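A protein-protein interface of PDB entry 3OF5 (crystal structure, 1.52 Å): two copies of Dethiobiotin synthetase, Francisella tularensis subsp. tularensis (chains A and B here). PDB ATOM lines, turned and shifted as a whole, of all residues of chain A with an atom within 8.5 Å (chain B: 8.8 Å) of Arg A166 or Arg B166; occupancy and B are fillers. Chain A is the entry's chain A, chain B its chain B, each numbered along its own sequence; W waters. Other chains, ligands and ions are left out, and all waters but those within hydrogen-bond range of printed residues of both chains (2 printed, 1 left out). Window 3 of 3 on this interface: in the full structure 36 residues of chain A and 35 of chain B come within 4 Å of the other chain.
Printed residues of chain A within 4 Å of Arg B166: Arg A166 (3.9 Å).
Of chain B, only Leu B159 (3.6 Å) and Asn B162 (3.0 Å) come within 4 Å of Glu A163.
Printed residues of chain B within 4 Å of Leu A123: Leu B158, Leu B159 and Asn B162.
Printed residues of chain A within 4 Å of Leu B158: Leu A123.
Printed residues of chain B within 4 Å of Asn A162: Leu B123 and Glu B163.
Ile B169 touches none of the printed residues of chain A.
Leu A133 touches none of the printed residues of chain B.
The nearest printed residue of chain B that does not touch Arg A166 is Leu B159 (4.3 Å).
The nearest printed residue of chain A that does not touch Leu B158 is Glu A163 (5.1 Å).
Leu A123 touches Leu B159, and with the chains exchanged Leu A159 touches Leu B123.
Asn A162 touches Glu B163, and with the chains exchanged Glu A163 touches Asn B162.
Arg A166 touches Glu B163, but with the chains exchanged Glu A163 does not touch Arg B166 (7.6 Å).
Arg B166 touches its own counterpart, Arg A166.
Hydrophobic or aromatic side chains of chain B within 4 Å of the printed part of chain A: Leu B123, Leu B158 and Leu B159.
Of the 17 printed residues of chain A, 7 touch a printed residue of chain B.
Printed residues of chain A that touch a printed residue of chain B: Leu A123, Leu A158, Leu A159, Thr A160, Asn A162, Glu A163 and Arg A166.
Among the printed residues, 16 pairs touch across the chains.
Among the printed residues, Asp or Glu carboxylates within 4 Å of a Lys or Arg side-chain nitrogen of the other chain: Arg A166 with Glu B163 (3.1 Å).
The side-chain carboxylate of Glu A163 sits at hydrogen-bond distance from the side-chain amide nitrogen of Asn B162, 3.0 Å away.
OE1 of Glu B163 sits at hydrogen-bond distance from ND2 of Asn A162 (3.0 Å).
The guanidinium group (NH1) of Arg A166 lies within salt-bridge range of the side-chain carboxylate (OE1) of Glu B163 (3.1 Å).
CD1 of Leu A123 touches CD2 of Leu B159, 3.7 Å away.
CD1 of Leu A123 touches ND2 of Asn B162 (3.5 Å).
Leu A158 touches Leu B123 (CB to CD1, 3.7 Å).
Leu A159 touches Leu B123 (CD2 to CD1, 3.7 Å).
Leu B159 touches Leu A159 (CD2 to O, 3.8 Å).
Thr B160 touches Leu A159 (OG1 to CD1, 3.7 Å).
Glu B163 touches Leu A159.
Leu B159 touches Thr A160 (CD1 to OG1, 3.7 Å).
Asn B162 touches Arg A166 (CB to NH2, 3.6 Å).
Arg A166 touches Arg B166 (NH1 to CB, 3.9 Å).
Water W2 lies within hydrogen-bond range of OE2 of Glu B163, NE2 of His B167 and ND2 of Asn A162.
Water W1 lies within hydrogen-bond range of OE2 of Glu A163 (2.7 Å), NE2 of His A167 (2.8 Å) and ND2 of Asn B162 (3.2 Å).
The side-chain carboxylate of Glu A163 lies within hydrogen-bond range of a ring nitrogen (NE2) of His A167, at 3.3 Å.
The guanidinium group (NH2) of Arg A166 is in salt-bridge range of the side-chain carboxylate (OE1) of Glu A163 (2.7 Å).
The backbone carbonyl oxygen (O) of Leu A158 lies close to the side-chain amide nitrogen (ND2) of Asn A162.
OE2 of Glu B163 is in hydrogen-bond range of NE2 of His B167 (3.3 Å).
O of Leu B158 sits close to OD1 of Asn B162 (3.4 Å).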
ATOM      1  N   LEU A 122      19.457  24.916  31.092  1.00  0.00           N
ATOM      2  CA  LEU A 122      20.895  25.018  30.816  1.00  0.00           C
ATOM      3  C   LEU A 122      21.300  26.375  30.286  1.00  0.00           C
ATOM      4  O   LEU A 122      22.352  26.897  30.681  1.00  0.00           O
ATOM      5  CB  LEU A 122      21.271  23.920  29.833  1.00  0.00           C
ATOM      6  CG  LEU A 122      22.730  23.809  29.464  1.00  0.00           C
ATOM      7  CD1 LEU A 122      23.633  23.754  30.734  1.00  0.00           C
ATOM      8  CD2 LEU A 122      22.937  22.589  28.629  1.00  0.00           C
ATOM      9  N   LEU A 123      20.492  26.918  29.374  1.00  0.00           N
ATOM     10  CA  LEU A 123      20.768  28.202  28.749  1.00  0.00           C
ATOM     11  C   LEU A 123      19.936  29.340  29.305  1.00  0.00           C
ATOM     12  O   LEU A 123      19.741  30.351  28.614  1.00  0.00           O
ATOM     13  CB  LEU A 123      20.703  28.106  27.236  1.00  0.00           C
ATOM     14  CG  LEU A 123      21.651  27.086  26.606  1.00  0.00           C
ATOM     15  CD1 LEU A 123      21.592  27.177  25.109  1.00  0.00           C
ATOM     16  CD2 LEU A 123      23.121  27.350  27.028  1.00  0.00           C
ATOM     17  N   LEU A 133      25.084  27.771  31.621  1.00  0.00           N
ATOM     18  CA  LEU A 133      26.121  26.920  31.052  1.00  0.00           C
ATOM     19  C   LEU A 133      27.526  27.510  31.262  1.00  0.00           C
ATOM     20  O   LEU A 133      28.440  26.756  31.585  1.00  0.00           O
ATOM     21  CB  LEU A 133      25.834  26.617  29.576  1.00  0.00           C
ATOM     22  CG  LEU A 133      26.830  25.691  28.878  1.00  0.00           C
ATOM     23  CD1 LEU A 133      26.141  24.775  27.893  1.00  0.00           C
ATOM     24  CD2 LEU A 133      27.917  26.488  28.186  1.00  0.00           C
ATOM     25  N   LYS A 137      30.437  25.356  32.888  1.00  0.00           N
ATOM     26  CA  LYS A 137      31.709  25.186  32.191  1.00  0.00           C
ATOM     27  C   LYS A 137      32.857  25.593  33.091  1.00  0.00           C
ATOM     28  O   LYS A 137      33.809  24.813  33.241  1.00  0.00           O
ATOM     29  CB  LYS A 137      31.745  26.057  30.926  1.00  0.00           C
ATOM     30  CG  LYS A 137      31.129  25.399  29.708  1.00  0.00           C
ATOM     31  CD  LYS A 137      31.547  26.112  28.421  1.00  0.00           C
ATOM     32  CE  LYS A 137      32.746  25.485  27.747  1.00  0.00           C
ATOM     33  NZ  LYS A 137      33.094  26.194  26.489  1.00  0.00           N
ATOM     34  N   LEU A 158      16.464  16.025  24.980  1.00  0.00           N
ATOM     35  CA  LEU A 158      17.507  15.764  23.985  1.00  0.00           C
ATOM     36  C   LEU A 158      18.281  17.046  23.655  1.00  0.00           C
ATOM     37  O   LEU A 158      19.512  17.003  23.506  1.00  0.00           O
ATOM     38  CB  LEU A 158      16.897  15.145  22.715  1.00  0.00           C
ATOM     39  CG  LEU A 158      16.206  13.803  22.879  1.00  0.00           C
ATOM     40  CD1 LEU A 158      15.685  13.334  21.543  1.00  0.00           C
ATOM     41  CD2 LEU A 158      17.171  12.763  23.483  1.00  0.00           C
ATOM     42  N   LEU A 159      17.577  18.181  23.523  1.00  0.00           N
ATOM     43  CA  LEU A 159      18.268  19.438  23.238  1.00  0.00           C
ATOM     44  C   LEU A 159      19.238  19.765  24.360  1.00  0.00           C
ATOM     45  O   LEU A 159      20.370  20.155  24.090  1.00  0.00           O
ATOM     46  CB  LEU A 159      17.288  20.601  23.091  1.00  0.00           C
ATOM     47  CG  LEU A 159      16.498  20.654  21.798  1.00  0.00           C
ATOM     48  CD1 LEU A 159      15.367  21.669  21.913  1.00  0.00           C
ATOM     49  CD2 LEU A 159      17.385  21.026  20.601  1.00  0.00           C
ATOM     50  N   THR A 160      18.808  19.580  25.619  1.00  0.00           N
ATOM     51  CA  THR A 160      19.687  19.884  26.762  1.00  0.00           C
ATOM     52  C   THR A 160      20.905  18.957  26.798  1.00  0.00           C
ATOM     53  O   THR A 160      22.029  19.433  26.966  1.00  0.00           O
ATOM     54  CB  THR A 160      18.893  19.821  28.079  1.00  0.00           C
ATOM     55  OG1 THR A 160      17.789  20.731  28.002  1.00  0.00           O
ATOM     56  CG2 THR A 160      19.747  20.148  29.297  1.00  0.00           C
ATOM     57  N   ILE A 161      20.688  17.643  26.611  1.00  0.00           N
ATOM     58  CA  ILE A 161      21.813  16.707  26.615  1.00  0.00           C
ATOM     59  C   ILE A 161      22.776  17.045  25.500  1.00  0.00           C
ATOM     60  O   ILE A 161      23.997  17.008  25.724  1.00  0.00           O
ATOM     61  CB  ILE A 161      21.302  15.245  26.547  1.00  0.00           C
ATOM     62  CG1 ILE A 161      20.575  14.892  27.856  1.00  0.00           C
ATOM     63  CG2 ILE A 161      22.456  14.237  26.261  1.00  0.00           C
ATOM     64  CD1 ILE A 161      19.818  13.542  27.842  1.00  0.00           C
ATOM     65  N   ASN A 162      22.263  17.363  24.292  1.00  0.00           N
ATOM     66  CA  ASN A 162      23.182  17.657  23.183  1.00  0.00           C
ATOM     67  C   ASN A 162      24.008  18.886  23.452  1.00  0.00           C
ATOM     68  O   ASN A 162      25.177  18.928  23.072  1.00  0.00           O
ATOM     69  CB  ASN A 162      22.429  17.810  21.866  1.00  0.00           C
ATOM     70  CG  ASN A 162      21.817  16.528  21.380  1.00  0.00           C
ATOM     71  OD1 ASN A 162      22.128  15.429  21.853  1.00  0.00           O
ATOM     72  ND2 ASN A 162      20.954  16.632  20.377  1.00  0.00           N
ATOM     73  N   GLU A 163      23.407  19.909  24.077  1.00  0.00           N
ATOM     74  CA  GLU A 163      24.160  21.112  24.389  1.00  0.00           C
ATOM     75  C   GLU A 163      25.277  20.806  25.402  1.00  0.00           C
ATOM     76  O   GLU A 163      26.413  21.272  25.237  1.00  0.00           O
ATOM     77  CB  GLU A 163      23.200  22.170  24.914  1.00  0.00           C
ATOM     78  CG  GLU A 163      23.835  23.516  25.245  1.00  0.00           C
ATOM     79  CD  GLU A 163      24.168  24.413  24.073  1.00  0.00           C
ATOM     80  OE1 GLU A 163      23.461  24.336  23.050  1.00  0.00           O
ATOM     81  OE2 GLU A 163      25.015  25.312  24.249  1.00  0.00           O
ATOM     82  N   LEU A 164      24.985  19.952  26.408  1.00  0.00           N
ATOM     83  CA  LEU A 164      26.026  19.544  27.377  1.00  0.00           C
ATOM     84  C   LEU A 164      27.167  18.836  26.640  1.00  0.00           C
ATOM     85  O   LEU A 164      28.334  19.157  26.879  1.00  0.00           O
ATOM     86  CB  LEU A 164      25.446  18.574  28.425  1.00  0.00           C
ATOM     87  CG  LEU A 164      24.444  19.163  29.419  1.00  0.00           C
ATOM     88  CD1 LEU A 164      23.821  18.063  30.278  1.00  0.00           C
ATOM     89  CD2 LEU A 164      25.100  20.208  30.331  1.00  0.00           C
ATOM     90  N   ASN A 165      26.825  17.889  25.748  1.00  0.00           N
ATOM     91  CA  ASN A 165      27.799  17.096  24.989  1.00  0.00           C
ATOM     92  C   ASN A 165      28.697  17.968  24.120  1.00  0.00           C
ATOM     93  O   ASN A 165      29.894  17.674  24.001  1.00  0.00           O
ATOM     94  CB  ASN A 165      27.090  16.058  24.125  1.00  0.00           C
ATOM     95  CG  ASN A 165      26.446  14.920  24.885  1.00  0.00           C
ATOM     96  OD1 ASN A 165      26.749  14.650  26.046  1.00  0.00           O
ATOM     97  ND2 ASN A 165      25.580  14.183  24.213  1.00  0.00           N
ATOM     98  N   ARG A 166      28.129  19.038  23.512  1.00  0.00           N
ATOM     99  CA  ARG A 166      28.885  19.958  22.648  1.00  0.00           C
ATOM    100  C   ARG A 166      29.954  20.693  23.437  1.00  0.00           C
ATOM    101  O   ARG A 166      31.062  20.884  22.928  1.00  0.00           O
ATOM    102  CB  ARG A 166      27.959  20.983  21.977  1.00  0.00           C
ATOM    103  CG  ARG A 166      27.113  20.407  20.839  1.00  0.00           C
ATOM    104  CD  ARG A 166      26.469  21.475  19.967  1.00  0.00           C
ATOM    105  NE  ARG A 166      25.351  22.152  20.628  1.00  0.00           N
ATOM    106  CZ  ARG A 166      24.084  21.778  20.514  1.00  0.00           C
ATOM    107  NH1 ARG A 166      23.767  20.694  19.817  1.00  0.00           N
ATOM    108  NH2 ARG A 166      23.130  22.444  21.151  1.00  0.00           N
ATOM    109  N   HIS A 167      29.630  21.083  24.685  1.00  0.00           N
ATOM    110  CA  HIS A 167      30.546  21.821  25.541  1.00  0.00           C
ATOM    111  C   HIS A 167      31.359  20.962  26.459  1.00  0.00           C
ATOM    112  O   HIS A 167      31.986  21.489  27.372  1.00  0.00           O
ATOM    113  CB  HIS A 167      29.816  22.930  26.293  1.00  0.00           C
ATOM    114  CG  HIS A 167      29.333  23.978  25.358  1.00  0.00           C
ATOM    115  ND1 HIS A 167      30.148  25.032  24.985  1.00  0.00           N
ATOM    116  CD2 HIS A 167      28.176  24.050  24.663  1.00  0.00           C
ATOM    117  CE1 HIS A 167      29.446  25.733  24.109  1.00  0.00           C
ATOM    118  NE2 HIS A 167      28.247  25.190  23.895  1.00  0.00           N
ATOM    119  N   ASN A 168      31.374  19.642  26.210  1.00  0.00           N
ATOM    120  CA  ASN A 168      32.185  18.685  26.969  1.00  0.00           C
ATOM    121  C   ASN A 168      31.876  18.707  28.462  1.00  0.00           C
ATOM    122  O   ASN A 168      32.790  18.681  29.306  1.00  0.00           O
ATOM    123  CB  ASN A 168      33.683  18.869  26.667  1.00  0.00           C
ATOM    124  CG  ASN A 168      34.514  17.661  27.016  1.00  0.00           C
ATOM    125  OD1 ASN A 168      34.057  16.516  26.907  1.00  0.00           O
ATOM    126  ND2 ASN A 168      35.715  17.888  27.525  1.00  0.00           N
ATOM    127  N   ILE A 169      30.571  18.790  28.806  1.00  0.00           N
ATOM    128  CA  ILE A 169      30.131  18.779  30.202  1.00  0.00           C
ATOM    129  C   ILE A 169      29.586  17.395  30.519  1.00  0.00           C
ATOM    130  O   ILE A 169      28.646  16.936  29.858  1.00  0.00           O
ATOM    131  CB  ILE A 169      29.100  19.893  30.497  1.00  0.00           C
ATOM    132  CG1 ILE A 169      29.711  21.293  30.325  1.00  0.00           C
ATOM    133  CG2 ILE A 169      28.505  19.726  31.911  1.00  0.00           C
ATOM    134  CD1 ILE A 169      28.586  22.429  30.079  1.00  0.00           C
ATOM    135  N   TYR A 199      21.452   7.566  27.046  1.00  0.00           N
ATOM    136  CA  TYR A 199      21.601   7.581  28.498  1.00  0.00           C
ATOM    137  C   TYR A 199      20.393   6.940  29.155  1.00  0.00           C
ATOM    138  O   TYR A 199      19.269   7.424  28.972  1.00  0.00           O
ATOM    139  CB  TYR A 199      21.726   9.025  29.030  1.00  0.00           C
ATOM    140  CG  TYR A 199      22.995   9.760  28.670  1.00  0.00           C
ATOM    141  CD1 TYR A 199      24.104   9.727  29.511  1.00  0.00           C
ATOM    142  CD2 TYR A 199      23.054  10.578  27.550  1.00  0.00           C
ATOM    143  CE1 TYR A 199      25.276  10.408  29.188  1.00  0.00           C
ATOM    144  CE2 TYR A 199      24.221  11.260  27.213  1.00  0.00           C
ATOM    145  CZ  TYR A 199      25.324  11.190  28.047  1.00  0.00           C
ATOM    146  OH  TYR A 199      26.465  11.896  27.747  1.00  0.00           O
ATOM    147  N   LEU B 122      12.235  20.769  17.439  1.00  0.00           N
ATOM    148  CA  LEU B 122      13.270  20.314  16.534  1.00  0.00           C
ATOM    149  C   LEU B 122      13.611  18.844  16.718  1.00  0.00           C
ATOM    150  O   LEU B 122      13.839  18.145  15.720  1.00  0.00           O
ATOM    151  CB  LEU B 122      14.518  21.196  16.730  1.00  0.00           C
ATOM    152  CG  LEU B 122      15.716  20.898  15.845  1.00  0.00           C
ATOM    153  CD1 LEU B 122      15.332  20.901  14.350  1.00  0.00           C
ATOM    154  CD2 LEU B 122      16.792  21.916  16.102  1.00  0.00           C
ATOM    155  N   LEU B 123      13.720  18.395  17.973  1.00  0.00           N
ATOM    156  CA  LEU B 123      14.055  17.018  18.278  1.00  0.00           C
ATOM    157  C   LEU B 123      12.852  16.199  18.702  1.00  0.00           C
ATOM    158  O   LEU B 123      13.024  15.194  19.388  1.00  0.00           O
ATOM    159  CB  LEU B 123      15.218  16.910  19.280  1.00  0.00           C
ATOM    160  CG  LEU B 123      16.531  17.597  18.837  1.00  0.00           C
ATOM    161  CD1 LEU B 123      17.655  17.385  19.844  1.00  0.00           C
ATOM    162  CD2 LEU B 123      17.018  17.071  17.473  1.00  0.00           C
ATOM    163  N   LEU B 133      14.563  16.683  13.156  1.00  0.00           N
ATOM    164  CA  LEU B 133      15.817  17.229  12.621  1.00  0.00           C
ATOM    165  C   LEU B 133      16.304  16.379  11.457  1.00  0.00           C
ATOM    166  O   LEU B 133      16.780  16.935  10.467  1.00  0.00           O
ATOM    167  CB  LEU B 133      16.908  17.260  13.697  1.00  0.00           C
ATOM    168  CG  LEU B 133      18.229  17.925  13.288  1.00  0.00           C
ATOM    169  CD1 LEU B 133      18.826  18.689  14.456  1.00  0.00           C
ATOM    170  CD2 LEU B 133      19.231  16.903  12.763  1.00  0.00           C
ATOM    171  N   LYS B 137      17.299  18.131   8.038  1.00  0.00           N
ATOM    172  CA  LYS B 137      18.666  18.005   7.542  1.00  0.00           C
ATOM    173  C   LYS B 137      18.694  17.321   6.168  1.00  0.00           C
ATOM    174  O   LYS B 137      19.465  17.746   5.293  1.00  0.00           O
ATOM    175  CB  LYS B 137      19.555  17.284   8.561  1.00  0.00           C
ATOM    176  CG  LYS B 137      21.027  17.507   8.309  1.00  0.00           C
ATOM    177  CD  LYS B 137      21.859  16.848   9.396  1.00  0.00           C
ATOM    178  CE  LYS B 137      23.308  17.201   9.224  1.00  0.00           C
ATOM    179  NZ  LYS B 137      24.153  16.596  10.293  1.00  0.00           N
ATOM    180  N   LEU B 158      17.297  29.367  22.609  1.00  0.00           N
ATOM    181  CA  LEU B 158      18.733  29.264  22.382  1.00  0.00           C
ATOM    182  C   LEU B 158      19.155  27.811  22.140  1.00  0.00           C
ATOM    183  O   LEU B 158      19.978  27.553  21.246  1.00  0.00           O
ATOM    184  CB  LEU B 158      19.527  29.865  23.571  1.00  0.00           C
ATOM    185  CG  LEU B 158      19.245  31.349  23.846  1.00  0.00           C
ATOM    186  CD1 LEU B 158      20.030  31.810  25.063  1.00  0.00           C
ATOM    187  CD2 LEU B 158      19.597  32.223  22.615  1.00  0.00           C
ATOM    188  N   LEU B 159      18.566  26.868  22.896  1.00  0.00           N
ATOM    189  CA  LEU B 159      18.906  25.459  22.683  1.00  0.00           C
ATOM    190  C   LEU B 159      18.567  25.044  21.248  1.00  0.00           C
ATOM    191  O   LEU B 159      19.353  24.335  20.597  1.00  0.00           O
ATOM    192  CB  LEU B 159      18.160  24.552  23.655  1.00  0.00           C
ATOM    193  CG  LEU B 159      18.664  24.527  25.097  1.00  0.00           C
ATOM    194  CD1 LEU B 159      17.677  23.799  25.985  1.00  0.00           C
ATOM    195  CD2 LEU B 159      20.011  23.807  25.218  1.00  0.00           C
ATOM    196  N   THR B 160      17.365  25.441  20.784  1.00  0.00           N
ATOM    197  CA  THR B 160      16.924  25.058  19.436  1.00  0.00           C
ATOM    198  C   THR B 160      17.849  25.696  18.388  1.00  0.00           C
ATOM    199  O   THR B 160      18.282  25.007  17.469  1.00  0.00           O
ATOM    200  CB  THR B 160      15.479  25.482  19.205  1.00  0.00           C
ATOM    201  OG1 THR B 160      14.625  24.876  20.187  1.00  0.00           O
ATOM    202  CG2 THR B 160      15.012  25.106  17.801  1.00  0.00           C
ATOM    203  N   ILE B 161      18.158  27.015  18.522  1.00  0.00           N
ATOM    204  CA  ILE B 161      19.039  27.688  17.580  1.00  0.00           C
ATOM    205  C   ILE B 161      20.417  26.978  17.559  1.00  0.00           C
ATOM    206  O   ILE B 161      21.003  26.774  16.486  1.00  0.00           O
ATOM    207  CB  ILE B 161      19.139  29.177  17.930  1.00  0.00           C
ATOM    208  CG1 ILE B 161      17.798  29.867  17.608  1.00  0.00           C
ATOM    209  CG2 ILE B 161      20.304  29.838  17.171  1.00  0.00           C
ATOM    210  CD1 ILE B 161      17.703  31.356  18.054  1.00  0.00           C
ATOM    211  N   ASN B 162      20.939  26.596  18.741  1.00  0.00           N
ATOM    212  CA  ASN B 162      22.239  25.939  18.764  1.00  0.00           C
ATOM    213  C   ASN B 162      22.244  24.593  18.094  1.00  0.00           C
ATOM    214  O   ASN B 162      23.240  24.255  17.421  1.00  0.00           O
ATOM    215  CB  ASN B 162      22.772  25.844  20.178  1.00  0.00           C
ATOM    216  CG  ASN B 162      23.065  27.186  20.783  1.00  0.00           C
ATOM    217  OD1 ASN B 162      23.146  28.230  20.093  1.00  0.00           O
ATOM    218  ND2 ASN B 162      23.343  27.184  22.074  1.00  0.00           N
ATOM    219  N   GLU B 163      21.155  23.818  18.264  1.00  0.00           N
ATOM    220  CA  GLU B 163      21.072  22.522  17.619  1.00  0.00           C
ATOM    221  C   GLU B 163      21.029  22.693  16.085  1.00  0.00           C
ATOM    222  O   GLU B 163      21.706  21.954  15.352  1.00  0.00           O
ATOM    223  CB  GLU B 163      19.837  21.788  18.134  1.00  0.00           C
ATOM    224  CG  GLU B 163      19.689  20.375  17.586  1.00  0.00           C
ATOM    225  CD  GLU B 163      20.587  19.311  18.181  1.00  0.00           C
ATOM    226  OE1 GLU B 163      20.992  19.449  19.356  1.00  0.00           O
ATOM    227  OE2 GLU B 163      20.795  18.284  17.501  1.00  0.00           O
ATOM    228  N   LEU B 164      20.294  23.713  15.608  1.00  0.00           N
ATOM    229  CA  LEU B 164      20.265  23.992  14.167  1.00  0.00           C
ATOM    230  C   LEU B 164      21.670  24.294  13.670  1.00  0.00           C
ATOM    231  O   LEU B 164      22.097  23.769  12.632  1.00  0.00           O
ATOM    232  CB  LEU B 164      19.366  25.193  13.871  1.00  0.00           C
ATOM    233  CG  LEU B 164      17.872  24.999  14.088  1.00  0.00           C
ATOM    234  CD1 LEU B 164      17.149  26.318  13.886  1.00  0.00           C
ATOM    235  CD2 LEU B 164      17.293  23.962  13.111  1.00  0.00           C
ATOM    236  N   ASN B 165      22.413  25.118  14.441  1.00  0.00           N
ATOM    237  CA  ASN B 165      23.776  25.510  14.052  1.00  0.00           C
ATOM    238  C   ASN B 165      24.670  24.272  13.975  1.00  0.00           C
ATOM    239  O   ASN B 165      25.410  24.084  12.992  1.00  0.00           O
ATOM    240  CB  ASN B 165      24.295  26.523  15.054  1.00  0.00           C
ATOM    241  CG  ASN B 165      25.638  27.122  14.709  1.00  0.00           C
ATOM    242  OD1 ASN B 165      26.194  26.922  13.628  1.00  0.00           O
ATOM    243  ND2 ASN B 165      26.182  27.888  15.638  1.00  0.00           N
ATOM    244  N   ARG B 166      24.552  23.382  14.954  1.00  0.00           N
ATOM    245  CA  ARG B 166      25.407  22.175  14.977  1.00  0.00           C
ATOM    246  C   ARG B 166      25.234  21.314  13.724  1.00  0.00           C
ATOM    247  O   ARG B 166      26.166  20.607  13.331  1.00  0.00           O
ATOM    248  CB  ARG B 166      25.090  21.338  16.234  1.00  0.00           C
ATOM    249  CG  ARG B 166      25.825  19.977  16.337  1.00  0.00           C
ATOM    250  CD  ARG B 166      27.338  20.122  16.401  1.00  0.00           C
ATOM    251  NE  ARG B 166      28.040  18.838  16.356  1.00  0.00           N
ATOM    252  CZ  ARG B 166      29.242  18.662  15.811  1.00  0.00           C
ATOM    253  NH1 ARG B 166      29.875  19.678  15.236  1.00  0.00           N
ATOM    254  NH2 ARG B 166      29.810  17.463  15.818  1.00  0.00           N
ATOM    255  N   HIS B 167      24.023  21.323  13.154  1.00  0.00           N
ATOM    256  CA  HIS B 167      23.698  20.515  11.982  1.00  0.00           C
ATOM    257  C   HIS B 167      23.639  21.310  10.698  1.00  0.00           C
ATOM    258  O   HIS B 167      23.182  20.782   9.676  1.00  0.00           O
ATOM    259  CB  HIS B 167      22.426  19.708  12.221  1.00  0.00           C
ATOM    260  CG  HIS B 167      22.651  18.663  13.257  1.00  0.00           C
ATOM    261  ND1 HIS B 167      23.312  17.488  12.951  1.00  0.00           N
ATOM    262  CD2 HIS B 167      22.401  18.690  14.586  1.00  0.00           C
ATOM    263  CE1 HIS B 167      23.415  16.822  14.090  1.00  0.00           C
ATOM    264  NE2 HIS B 167      22.883  17.503  15.101  1.00  0.00           N
ATOM    265  N   ASN B 168      24.150  22.557  10.726  1.00  0.00           N
ATOM    266  CA  ASN B 168      24.236  23.440   9.558  1.00  0.00           C
ATOM    267  C   ASN B 168      22.903  23.602   8.858  1.00  0.00           C
ATOM    268  O   ASN B 168      22.819  23.558   7.626  1.00  0.00           O
ATOM    269  CB  ASN B 168      25.367  22.999   8.604  1.00  0.00           C
ATOM    270  CG  ASN B 168      26.690  23.129   9.289  1.00  0.00           C
ATOM    271  OD1 ASN B 168      26.912  24.065  10.058  1.00  0.00           O
ATOM    272  ND2 ASN B 168      27.574  22.187   9.070  1.00  0.00           N
ATOM    273  N   ILE B 169      21.858  23.784   9.668  1.00  0.00           N
ATOM    274  CA  ILE B 169      20.514  24.033   9.150  1.00  0.00           C
ATOM    275  C   ILE B 169      20.320  25.542   9.290  1.00  0.00           C
ATOM    276  O   ILE B 169      20.359  26.072  10.404  1.00  0.00           O
ATOM    277  CB  ILE B 169      19.443  23.242   9.920  1.00  0.00           C
ATOM    278  CG1 ILE B 169      19.636  21.720   9.755  1.00  0.00           C
ATOM    279  CG2 ILE B 169      18.047  23.679   9.441  1.00  0.00           C
ATOM    280  CD1 ILE B 169      18.802  20.865  10.785  1.00  0.00           C
ATOM    281  N   LYS B 170      20.111  26.236   8.161  1.00  0.00           N
ATOM    282  CA  LYS B 170      19.968  27.682   8.180  1.00  0.00           C
ATOM    283  C   LYS B 170      18.732  28.111   8.936  1.00  0.00           C
ATOM    284  O   LYS B 170      17.652  27.544   8.730  1.00  0.00           O
ATOM    285  CB  LYS B 170      19.874  28.209   6.743  1.00  0.00           C
ATOM    286  CG  LYS B 170      19.812  29.729   6.658  1.00  0.00           C
ATOM    287  CD  LYS B 170      19.814  30.235   5.232  1.00  0.00           C
ATOM    288  CE  LYS B 170      19.839  31.748   5.197  1.00  0.00           C
ATOM    289  NZ  LYS B 170      21.168  32.293   5.597  1.00  0.00           N
HETATM  290  O   HOH W   1      26.387  26.136  22.096  1.00  0.00           O
HETATM  291  O   HOH W   2      23.031  16.912  17.867  1.00  0.00           O
